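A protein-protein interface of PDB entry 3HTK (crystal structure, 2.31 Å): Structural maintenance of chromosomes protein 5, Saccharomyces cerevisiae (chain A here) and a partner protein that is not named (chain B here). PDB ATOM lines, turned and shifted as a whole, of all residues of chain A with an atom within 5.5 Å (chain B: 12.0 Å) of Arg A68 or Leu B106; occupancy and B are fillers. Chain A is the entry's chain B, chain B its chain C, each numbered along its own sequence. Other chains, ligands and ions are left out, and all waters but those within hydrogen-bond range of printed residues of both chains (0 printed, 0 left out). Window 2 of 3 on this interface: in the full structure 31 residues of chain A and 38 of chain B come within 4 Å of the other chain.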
ATOM      1  N   VAL A  61      11.010  20.762  27.438  1.00  0.00           N
ATOM      2  CA  VAL A  61      11.286  20.014  26.214  1.00  0.00           C
ATOM      3  C   VAL A  61      12.739  20.106  25.774  1.00  0.00           C
ATOM      4  O   VAL A  61      13.343  19.098  25.422  1.00  0.00           O
ATOM      5  CB  VAL A  61      10.374  20.463  25.067  1.00  0.00           C
ATOM      6  CG1 VAL A  61      10.773  19.779  23.786  1.00  0.00           C
ATOM      7  CG2 VAL A  61       8.939  20.110  25.402  1.00  0.00           C
ATOM      8  N   PHE A  64      14.810  17.931  27.794  1.00  0.00           N
ATOM      9  CA  PHE A  64      14.696  16.534  27.405  1.00  0.00           C
ATOM     10  C   PHE A  64      15.438  16.276  26.104  1.00  0.00           C
ATOM     11  O   PHE A  64      16.095  15.248  25.952  1.00  0.00           O
ATOM     12  CB  PHE A  64      13.221  16.127  27.268  1.00  0.00           C
ATOM     13  CG  PHE A  64      12.452  16.198  28.559  1.00  0.00           C
ATOM     14  CD1 PHE A  64      13.056  15.837  29.768  1.00  0.00           C
ATOM     15  CD2 PHE A  64      11.120  16.606  28.569  1.00  0.00           C
ATOM     16  CE1 PHE A  64      12.342  15.881  30.971  1.00  0.00           C
ATOM     17  CE2 PHE A  64      10.394  16.653  29.759  1.00  0.00           C
ATOM     18  CZ  PHE A  64      11.002  16.291  30.964  1.00  0.00           C
ATOM     19  N   PHE A  65      15.337  17.212  25.170  1.00  0.00           N
ATOM     20  CA  PHE A  65      16.020  17.070  23.894  1.00  0.00           C
ATOM     21  C   PHE A  65      17.517  16.859  24.109  1.00  0.00           C
ATOM     22  O   PHE A  65      18.101  15.933  23.549  1.00  0.00           O
ATOM     23  CB  PHE A  65      15.818  18.314  23.034  1.00  0.00           C
ATOM     24  CG  PHE A  65      16.366  18.181  21.642  1.00  0.00           C
ATOM     25  CD1 PHE A  65      15.559  17.719  20.605  1.00  0.00           C
ATOM     26  CD2 PHE A  65      17.691  18.505  21.369  1.00  0.00           C
ATOM     27  CE1 PHE A  65      16.065  17.581  19.311  1.00  0.00           C
ATOM     28  CE2 PHE A  65      18.211  18.373  20.082  1.00  0.00           C
ATOM     29  CZ  PHE A  65      17.396  17.911  19.050  1.00  0.00           C
ATOM     30  N   ASN A  66      18.129  17.721  24.922  1.00  0.00           N
ATOM     31  CA  ASN A  66      19.564  17.635  25.195  1.00  0.00           C
ATOM     32  C   ASN A  66      19.996  16.336  25.866  1.00  0.00           C
ATOM     33  O   ASN A  66      21.191  16.031  25.921  1.00  0.00           O
ATOM     34  CB  ASN A  66      20.034  18.812  26.057  1.00  0.00           C
ATOM     35  CG  ASN A  66      19.979  20.134  25.324  1.00  0.00           C
ATOM     36  OD1 ASN A  66      20.082  20.186  24.096  1.00  0.00           O
ATOM     37  ND2 ASN A  66      19.840  21.220  26.078  1.00  0.00           N
ATOM     38  N   GLU A  67      19.037  15.580  26.386  1.00  0.00           N
ATOM     39  CA  GLU A  67      19.365  14.320  27.034  1.00  0.00           C
ATOM     40  C   GLU A  67      19.578  13.264  25.968  1.00  0.00           C
ATOM     41  O   GLU A  67      20.605  12.592  25.956  1.00  0.00           O
ATOM     42  CB  GLU A  67      18.248  13.887  27.980  1.00  0.00           C
ATOM     43  CG  GLU A  67      18.119  14.751  29.219  1.00  0.00           C
ATOM     44  CD  GLU A  67      16.947  14.336  30.084  1.00  0.00           C
ATOM     45  OE1 GLU A  67      16.946  13.183  30.573  1.00  0.00           O
ATOM     46  OE2 GLU A  67      16.027  15.163  30.273  1.00  0.00           O
ATOM     47  N   ARG A  68      18.612  13.136  25.063  1.00  0.00           N
ATOM     48  CA  ARG A  68      18.698  12.165  23.977  1.00  0.00           C
ATOM     49  C   ARG A  68      20.002  12.277  23.201  1.00  0.00           C
ATOM     50  O   ARG A  68      20.334  11.389  22.419  1.00  0.00           O
ATOM     51  CB  ARG A  68      17.536  12.337  23.000  1.00  0.00           C
ATOM     52  CG  ARG A  68      16.234  11.715  23.445  1.00  0.00           C
ATOM     53  CD  ARG A  68      15.238  11.733  22.301  1.00  0.00           C
ATOM     54  NE  ARG A  68      13.923  11.247  22.706  1.00  0.00           N
ATOM     55  CZ  ARG A  68      12.840  11.297  21.936  1.00  0.00           C
ATOM     56  NH1 ARG A  68      12.918  11.810  20.713  1.00  0.00           N
ATOM     57  NH2 ARG A  68      11.675  10.849  22.391  1.00  0.00           N
ATOM     58  N   GLU A  69      20.730  13.371  23.409  1.00  0.00           N
ATOM     59  CA  GLU A  69      21.996  13.590  22.718  1.00  0.00           C
ATOM     60  C   GLU A  69      23.193  13.266  23.609  1.00  0.00           C
ATOM     61  O   GLU A  69      24.067  12.487  23.227  1.00  0.00           O
ATOM     62  CB  GLU A  69      22.096  15.042  22.244  1.00  0.00           C
ATOM     63  CG  GLU A  69      21.037  15.459  21.230  1.00  0.00           C
ATOM     64  CD  GLU A  69      21.132  14.690  19.925  1.00  0.00           C
ATOM     65  OE1 GLU A  69      22.236  14.638  19.342  1.00  0.00           O
ATOM     66  OE2 GLU A  69      20.101  14.143  19.479  1.00  0.00           O
ATOM     67  N   ALA A  70      23.224  13.863  24.797  1.00  0.00           N
ATOM     68  CA  ALA A  70      24.318  13.655  25.741  1.00  0.00           C
ATOM     69  C   ALA A  70      24.450  12.210  26.224  1.00  0.00           C
ATOM     70  O   ALA A  70      25.470  11.840  26.810  1.00  0.00           O
ATOM     71  CB  ALA A  70      24.159  14.592  26.939  1.00  0.00           C
ATOM     72  N   ASP A  71      23.423  11.398  25.989  1.00  0.00           N
ATOM     73  CA  ASP A  71      23.462  10.000  26.409  1.00  0.00           C
ATOM     74  C   ASP A  71      23.639   9.104  25.185  1.00  0.00           C
ATOM     75  O   ASP A  71      24.231   8.028  25.269  1.00  0.00           O
ATOM     76  CB  ASP A  71      22.169   9.617  27.134  1.00  0.00           C
ATOM     77  CG  ASP A  71      21.105   9.087  26.188  1.00  0.00           C
ATOM     78  OD1 ASP A  71      20.682   9.831  25.279  1.00  0.00           O
ATOM     79  OD2 ASP A  71      20.693   7.918  26.351  1.00  0.00           O
ATOM     80  N   LEU A  72      23.115   9.562  24.051  1.00  0.00           N
ATOM     81  CA  LEU A  72      23.199   8.827  22.794  1.00  0.00           C
ATOM     82  C   LEU A  72      24.654   8.545  22.443  1.00  0.00           C
ATOM     83  O   LEU A  72      24.962   7.583  21.738  1.00  0.00           O
ATOM     84  CB  LEU A  72      22.542   9.641  21.675  1.00  0.00           C
ATOM     85  CG  LEU A  72      22.506   9.079  20.251  1.00  0.00           C
ATOM     86  CD1 LEU A  72      21.699   7.787  20.212  1.00  0.00           C
ATOM     87  CD2 LEU A  72      21.889  10.116  19.324  1.00  0.00           C
ATOM     88  N   PRO B   7       6.761  26.277  14.422  1.00  0.00           N
ATOM     89  CA  PRO B   7       7.758  25.824  15.402  1.00  0.00           C
ATOM     90  C   PRO B   7       7.231  25.762  16.835  1.00  0.00           C
ATOM     91  O   PRO B   7       7.721  24.979  17.652  1.00  0.00           O
ATOM     92  CB  PRO B   7       8.887  26.841  15.238  1.00  0.00           C
ATOM     93  CG  PRO B   7       8.151  28.092  14.847  1.00  0.00           C
ATOM     94  CD  PRO B   7       7.161  27.566  13.829  1.00  0.00           C
ATOM     95  N   PRO B   9       3.697  25.369  19.282  1.00  0.00           N
ATOM     96  CA  PRO B   9       2.295  24.946  19.290  1.00  0.00           C
ATOM     97  C   PRO B   9       1.307  26.089  19.542  1.00  0.00           C
ATOM     98  O   PRO B   9       1.666  27.119  20.124  1.00  0.00           O
ATOM     99  CB  PRO B   9       2.267  23.884  20.392  1.00  0.00           C
ATOM    100  CG  PRO B   9       3.318  24.348  21.329  1.00  0.00           C
ATOM    101  CD  PRO B   9       4.437  24.740  20.390  1.00  0.00           C
ATOM    102  N   VAL B  12      -0.403  24.960  24.953  1.00  0.00           N
ATOM    103  CA  VAL B  12       0.076  23.842  25.736  1.00  0.00           C
ATOM    104  C   VAL B  12      -0.704  23.929  27.032  1.00  0.00           C
ATOM    105  O   VAL B  12      -1.283  24.976  27.338  1.00  0.00           O
ATOM    106  CB  VAL B  12       1.615  23.917  26.009  1.00  0.00           C
ATOM    107  CG1 VAL B  12       2.378  23.752  24.695  1.00  0.00           C
ATOM    108  CG2 VAL B  12       1.984  25.221  26.705  1.00  0.00           C
ATOM    109  N   PRO B  13      -0.768  22.829  27.792  1.00  0.00           N
ATOM    110  CA  PRO B  13      -1.505  22.836  29.060  1.00  0.00           C
ATOM    111  C   PRO B  13      -0.847  23.657  30.153  1.00  0.00           C
ATOM    112  O   PRO B  13       0.261  24.161  29.976  1.00  0.00           O
ATOM    113  CB  PRO B  13      -1.590  21.339  29.431  1.00  0.00           C
ATOM    114  CG  PRO B  13      -0.395  20.750  28.758  1.00  0.00           C
ATOM    115  CD  PRO B  13      -0.349  21.462  27.427  1.00  0.00           C
ATOM    116  N   HIS B  15       1.312  24.376  33.047  1.00  0.00           N
ATOM    117  CA  HIS B  15       2.507  23.767  33.607  1.00  0.00           C
ATOM    118  C   HIS B  15       2.495  23.914  35.122  1.00  0.00           C
ATOM    119  O   HIS B  15       2.068  24.938  35.647  1.00  0.00           O
ATOM    120  CB  HIS B  15       3.740  24.455  33.040  1.00  0.00           C
ATOM    121  CG  HIS B  15       5.019  23.769  33.382  1.00  0.00           C
ATOM    122  ND1 HIS B  15       5.668  22.928  32.505  1.00  0.00           N
ATOM    123  CD2 HIS B  15       5.758  23.778  34.518  1.00  0.00           C
ATOM    124  CE1 HIS B  15       6.756  22.452  33.085  1.00  0.00           C
ATOM    125  NE2 HIS B  15       6.833  22.951  34.307  1.00  0.00           N
ATOM    126  N   PRO B 102      -2.266  15.842  28.453  1.00  0.00           N
ATOM    127  CA  PRO B 102      -0.993  15.215  28.806  1.00  0.00           C
ATOM    128  C   PRO B 102       0.074  16.290  28.999  1.00  0.00           C
ATOM    129  O   PRO B 102       0.059  17.305  28.305  1.00  0.00           O
ATOM    130  CB  PRO B 102      -0.707  14.329  27.595  1.00  0.00           C
ATOM    131  CG  PRO B 102      -2.085  13.892  27.178  1.00  0.00           C
ATOM    132  CD  PRO B 102      -2.843  15.206  27.249  1.00  0.00           C
ATOM    133  N   GLN B 103       0.980  16.078  29.952  1.00  0.00           N
ATOM    134  CA  GLN B 103       2.050  17.037  30.209  1.00  0.00           C
ATOM    135  C   GLN B 103       2.923  17.093  28.976  1.00  0.00           C
ATOM    136  O   GLN B 103       2.869  16.216  28.113  1.00  0.00           O
ATOM    137  CB  GLN B 103       2.941  16.606  31.373  1.00  0.00           C
ATOM    138  CG  GLN B 103       2.335  16.636  32.750  1.00  0.00           C
ATOM    139  CD  GLN B 103       3.210  15.880  33.759  1.00  0.00           C
ATOM    140  OE1 GLN B 103       3.316  14.651  33.702  1.00  0.00           O
ATOM    141  NE2 GLN B 103       3.852  16.615  34.670  1.00  0.00           N
ATOM    142  N   ILE B 104       3.759  18.117  28.921  1.00  0.00           N
ATOM    143  CA  ILE B 104       4.647  18.304  27.799  1.00  0.00           C
ATOM    144  C   ILE B 104       5.908  17.455  27.947  1.00  0.00           C
ATOM    145  O   ILE B 104       6.505  17.398  29.022  1.00  0.00           O
ATOM    146  CB  ILE B 104       5.034  19.792  27.677  1.00  0.00           C
ATOM    147  CG1 ILE B 104       5.258  20.147  26.213  1.00  0.00           C
ATOM    148  CG2 ILE B 104       6.267  20.089  28.518  1.00  0.00           C
ATOM    149  CD1 ILE B 104       3.993  20.059  25.390  1.00  0.00           C
ATOM    150  N   ASP B 105       6.284  16.769  26.872  1.00  0.00           N
ATOM    151  CA  ASP B 105       7.499  15.962  26.854  1.00  0.00           C
ATOM    152  C   ASP B 105       7.954  15.792  25.402  1.00  0.00           C
ATOM    153  O   ASP B 105       7.303  16.302  24.485  1.00  0.00           O
ATOM    154  CB  ASP B 105       7.287  14.606  27.571  1.00  0.00           C
ATOM    155  CG  ASP B 105       6.297  13.683  26.864  1.00  0.00           C
ATOM    156  OD1 ASP B 105       5.898  12.685  27.496  1.00  0.00           O
ATOM    157  OD2 ASP B 105       5.922  13.923  25.698  1.00  0.00           O
ATOM    158  N   LEU B 106       9.067  15.100  25.184  1.00  0.00           N
ATOM    159  CA  LEU B 106       9.590  14.923  23.830  1.00  0.00           C
ATOM    160  C   LEU B 106       8.575  14.481  22.773  1.00  0.00           C
ATOM    161  O   LEU B 106       8.638  14.937  21.627  1.00  0.00           O
ATOM    162  CB  LEU B 106      10.788  13.968  23.852  1.00  0.00           C
ATOM    163  CG  LEU B 106      12.079  14.617  24.368  1.00  0.00           C
ATOM    164  CD1 LEU B 106      13.170  13.581  24.575  1.00  0.00           C
ATOM    165  CD2 LEU B 106      12.516  15.680  23.374  1.00  0.00           C
ATOM    166  N   SER B 107       7.638  13.612  23.143  1.00  0.00           N
ATOM    167  CA  SER B 107       6.624  13.154  22.189  1.00  0.00           C
ATOM    168  C   SER B 107       5.438  14.119  22.156  1.00  0.00           C
ATOM    169  O   SER B 107       5.016  14.581  21.099  1.00  0.00           O
ATOM    170  CB  SER B 107       6.121  11.756  22.572  1.00  0.00           C
ATOM    171  OG  SER B 107       5.422  11.777  23.807  1.00  0.00           O
ATOM    172  N   THR B 108       4.910  14.401  23.341  1.00  0.00           N
ATOM    173  CA  THR B 108       3.782  15.297  23.530  1.00  0.00           C
ATOM    174  C   THR B 108       3.973  16.664  22.862  1.00  0.00           C
ATOM    175  O   THR B 108       3.052  17.183  22.235  1.00  0.00           O
ATOM    176  CB  THR B 108       3.515  15.468  25.049  1.00  0.00           C
ATOM    177  OG1 THR B 108       2.746  14.356  25.522  1.00  0.00           O
ATOM    178  CG2 THR B 108       2.786  16.739  25.336  1.00  0.00           C
ATOM    179  N   TRP B 109       5.162  17.247  22.983  1.00  0.00           N
ATOM    180  CA  TRP B 109       5.413  18.553  22.377  1.00  0.00           C
ATOM    181  C   TRP B 109       5.135  18.622  20.877  1.00  0.00           C
ATOM    182  O   TRP B 109       4.656  19.647  20.385  1.00  0.00           O
ATOM    183  CB  TRP B 109       6.850  19.012  22.642  1.00  0.00           C
ATOM    184  CG  TRP B 109       7.209  20.272  21.902  1.00  0.00           C
ATOM    185  CD1 TRP B 109       7.587  20.375  20.592  1.00  0.00           C
ATOM    186  CD2 TRP B 109       7.187  21.607  22.419  1.00  0.00           C
ATOM    187  NE1 TRP B 109       7.802  21.691  20.263  1.00  0.00           N
ATOM    188  CE2 TRP B 109       7.567  22.470  21.365  1.00  0.00           C
ATOM    189  CE3 TRP B 109       6.885  22.160  23.671  1.00  0.00           C
ATOM    190  CZ2 TRP B 109       7.656  23.862  21.525  1.00  0.00           C
ATOM    191  CZ3 TRP B 109       6.974  23.547  23.833  1.00  0.00           C
ATOM    192  CH2 TRP B 109       7.358  24.379  22.761  1.00  0.00           C
ATOM    193  N   ASP B 110       5.445  17.555  20.142  1.00  0.00           N
ATOM    194  CA  ASP B 110       5.189  17.551  18.700  1.00  0.00           C
ATOM    195  C   ASP B 110       3.700  17.458  18.428  1.00  0.00           C
ATOM    196  O   ASP B 110       3.198  18.069  17.481  1.00  0.00           O
ATOM    197  CB  ASP B 110       5.897  16.382  18.007  1.00  0.00           C
ATOM    198  CG  ASP B 110       7.368  16.650  17.771  1.00  0.00           C
ATOM    199  OD1 ASP B 110       8.159  16.571  18.739  1.00  0.00           O
ATOM    200  OD2 ASP B 110       7.724  16.952  16.610  1.00  0.00           O
ATOM    201  N   LYS B 111       3.004  16.677  19.253  1.00  0.00           N
ATOM    202  CA  LYS B 111       1.560  16.520  19.110  1.00  0.00           C
ATOM    203  C   LYS B 111       0.835  17.857  19.343  1.00  0.00           C
ATOM    204  O   LYS B 111      -0.064  18.214  18.577  1.00  0.00           O
ATOM    205  CB  LYS B 111       1.038  15.452  20.074  1.00  0.00           C
ATOM    206  CG  LYS B 111       1.458  14.028  19.714  1.00  0.00           C
ATOM    207  CD  LYS B 111       0.952  13.020  20.737  1.00  0.00           C
ATOM    208  CE  LYS B 111       1.307  11.587  20.341  1.00  0.00           C
ATOM    209  NZ  LYS B 111       0.592  11.141  19.110  1.00  0.00           N
ATOM    210  N   TYR B 112       1.220  18.600  20.383  1.00  0.00           N
ATOM    211  CA  TYR B 112       0.573  19.889  20.622  1.00  0.00           C
ATOM    212  C   TYR B 112       0.859  20.865  19.483  1.00  0.00           C
ATOM    213  O   TYR B 112       0.042  21.728  19.179  1.00  0.00           O
ATOM    214  CB  TYR B 112       1.024  20.495  21.947  1.00  0.00           C
ATOM    215  CG  TYR B 112       0.329  19.879  23.134  1.00  0.00           C
ATOM    216  CD1 TYR B 112      -1.040  20.065  23.344  1.00  0.00           C
ATOM    217  CD2 TYR B 112       1.031  19.087  24.037  1.00  0.00           C
ATOM    218  CE1 TYR B 112      -1.686  19.473  24.427  1.00  0.00           C
ATOM    219  CE2 TYR B 112       0.396  18.492  25.112  1.00  0.00           C
ATOM    220  CZ  TYR B 112      -0.958  18.685  25.309  1.00  0.00           C
ATOM    221  OH  TYR B 112      -1.559  18.095  26.401  1.00  0.00           O
ATOM    222  N   ARG B 113       2.015  20.709  18.844  1.00  0.00           N
ATOM    223  CA  ARG B 113       2.400  21.574  17.739  1.00  0.00           C
ATOM    224  C   ARG B 113       1.645  21.226  16.461  1.00  0.00           C
ATOM    225  O   ARG B 113       1.190  22.104  15.727  1.00  0.00           O
ATOM    226  CB  ARG B 113       3.904  21.459  17.501  1.00  0.00           C
ATOM    227  CG  ARG B 113       4.425  22.435  16.474  1.00  0.00           C
ATOM    228  CD  ARG B 113       5.932  22.527  16.542  1.00  0.00           C
ATOM    229  NE  ARG B 113       6.565  21.275  16.162  1.00  0.00           N
ATOM    230  CZ  ARG B 113       7.879  21.099  16.117  1.00  0.00           C
ATOM    231  NH1 ARG B 113       8.690  22.103  16.432  1.00  0.00           N
ATOM    232  NH2 ARG B 113       8.379  19.927  15.749  1.00  0.00           N
ATOM    233  N   THR B 114       1.517  19.926  16.213  1.00  0.00           N
ATOM    234  CA  THR B 114       0.827  19.393  15.041  1.00  0.00           C
ATOM    235  C   THR B 114      -0.706  19.486  15.146  1.00  0.00           C
ATOM    236  O   THR B 114      -1.410  19.563  14.134  1.00  0.00           O
ATOM    237  CB  THR B 114       1.227  17.915  14.827  1.00  0.00           C
ATOM    238  OG1 THR B 114       0.679  17.439  13.594  1.00  0.00           O
ATOM    239  CG2 THR B 114       0.708  17.058  15.953  1.00  0.00           C
ATOM    240  N   GLU B 116      -2.501  17.159  17.048  1.00  0.00           N
ATOM    241  CA  GLU B 116      -2.991  15.870  17.540  1.00  0.00           C
ATOM    242  C   GLU B 116      -3.564  16.095  18.921  1.00  0.00           C
ATOM    243  O   GLU B 116      -4.687  15.690  19.203  1.00  0.00           O
ATOM    244  CB  GLU B 116      -1.865  14.833  17.597  1.00  0.00           C
ATOM    245  CG  GLU B 116      -1.315  14.449  16.228  1.00  0.00           C
ATOM    246  CD  GLU B 116      -0.256  13.368  16.310  1.00  0.00           C
ATOM    247  OE1 GLU B 116      -0.603  12.226  16.682  1.00  0.00           O
ATOM    248  OE2 GLU B 116       0.921  13.662  16.008  1.00  0.00           O
ATOM    249  N   LEU B 117      -2.785  16.731  19.786  1.00  0.00           N
ATOM    250  CA  LEU B 117      -3.263  17.060  21.121  1.00  0.00           C
ATOM    251  C   LEU B 117      -3.549  18.552  21.060  1.00  0.00           C
ATOM    252  O   LEU B 117      -2.841  19.297  20.369  1.00  0.00           O
ATOM    253  CB  LEU B 117      -2.202  16.783  22.188  1.00  0.00           C
ATOM    254  CG  LEU B 117      -1.851  15.321  22.473  1.00  0.00           C
ATOM    255  CD1 LEU B 117      -0.709  15.212  23.489  1.00  0.00           C
ATOM    256  CD2 LEU B 117      -3.060  14.627  22.998  1.00  0.00           C
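Among the printed residues, merely in contact across the chains: Arg A68 with Leu B106 (3.1 Å), Val A61 with Trp B109 (3.4 Å), Phe A64 with Leu B106 (3.5 Å), Phe A65 with Leu B106 (3.7 Å) and Val A61 with Ile B104 (3.8 Å).
Leu B106 touches just these residues of chain A: Phe A64, Phe A65 and Arg A68. Of chain B, only Ile B104 and Trp B109 come within 4 Å of Val A61. Printed residues of chain B within 4 Å of Phe A64: Leu B106 (3.5 Å). Phe A65 touches just one residue of chain B: Leu B106. Glu A67 touches none of the printed residues of chain B. No residue of chain B comes within 4 Å of Asp A71. No residue of chain B comes within 4 Å of Leu A72. Of the printed residues of chain A, Trp B109 touches Val A61 (3.4 Å). Of the printed residues of chain A, Ile B104 touches Val A61 (3.8 Å). Glu B116 touches none of the printed residues of chain A. The nearest residue of chain B that does not touch Arg A68 is Ser B107 (4.9 Å). The nearest residue of chain A that does not touch Leu B106 is Val A61 (4.1 Å). The nearest printed residue of chain A that does not touch Ile B104 is Phe A64 (4.03 Å).
Printed residues of chain A that touch a printed residue of chain B: Val A61, Phe A64, Phe A65 and Arg A68. Along chain A the printed residues that touch a printed residue of chain B span positions 61 to 68. Of the 20 printed residues of chain B, 3 touch a printed residue of chain A. Among the printed residues, 5 pairs touch across the chains. Among the printed residues, no Asp or Glu carboxylate lies within 4 Å of a Lys or Arg side-chain nitrogen of the other chain.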
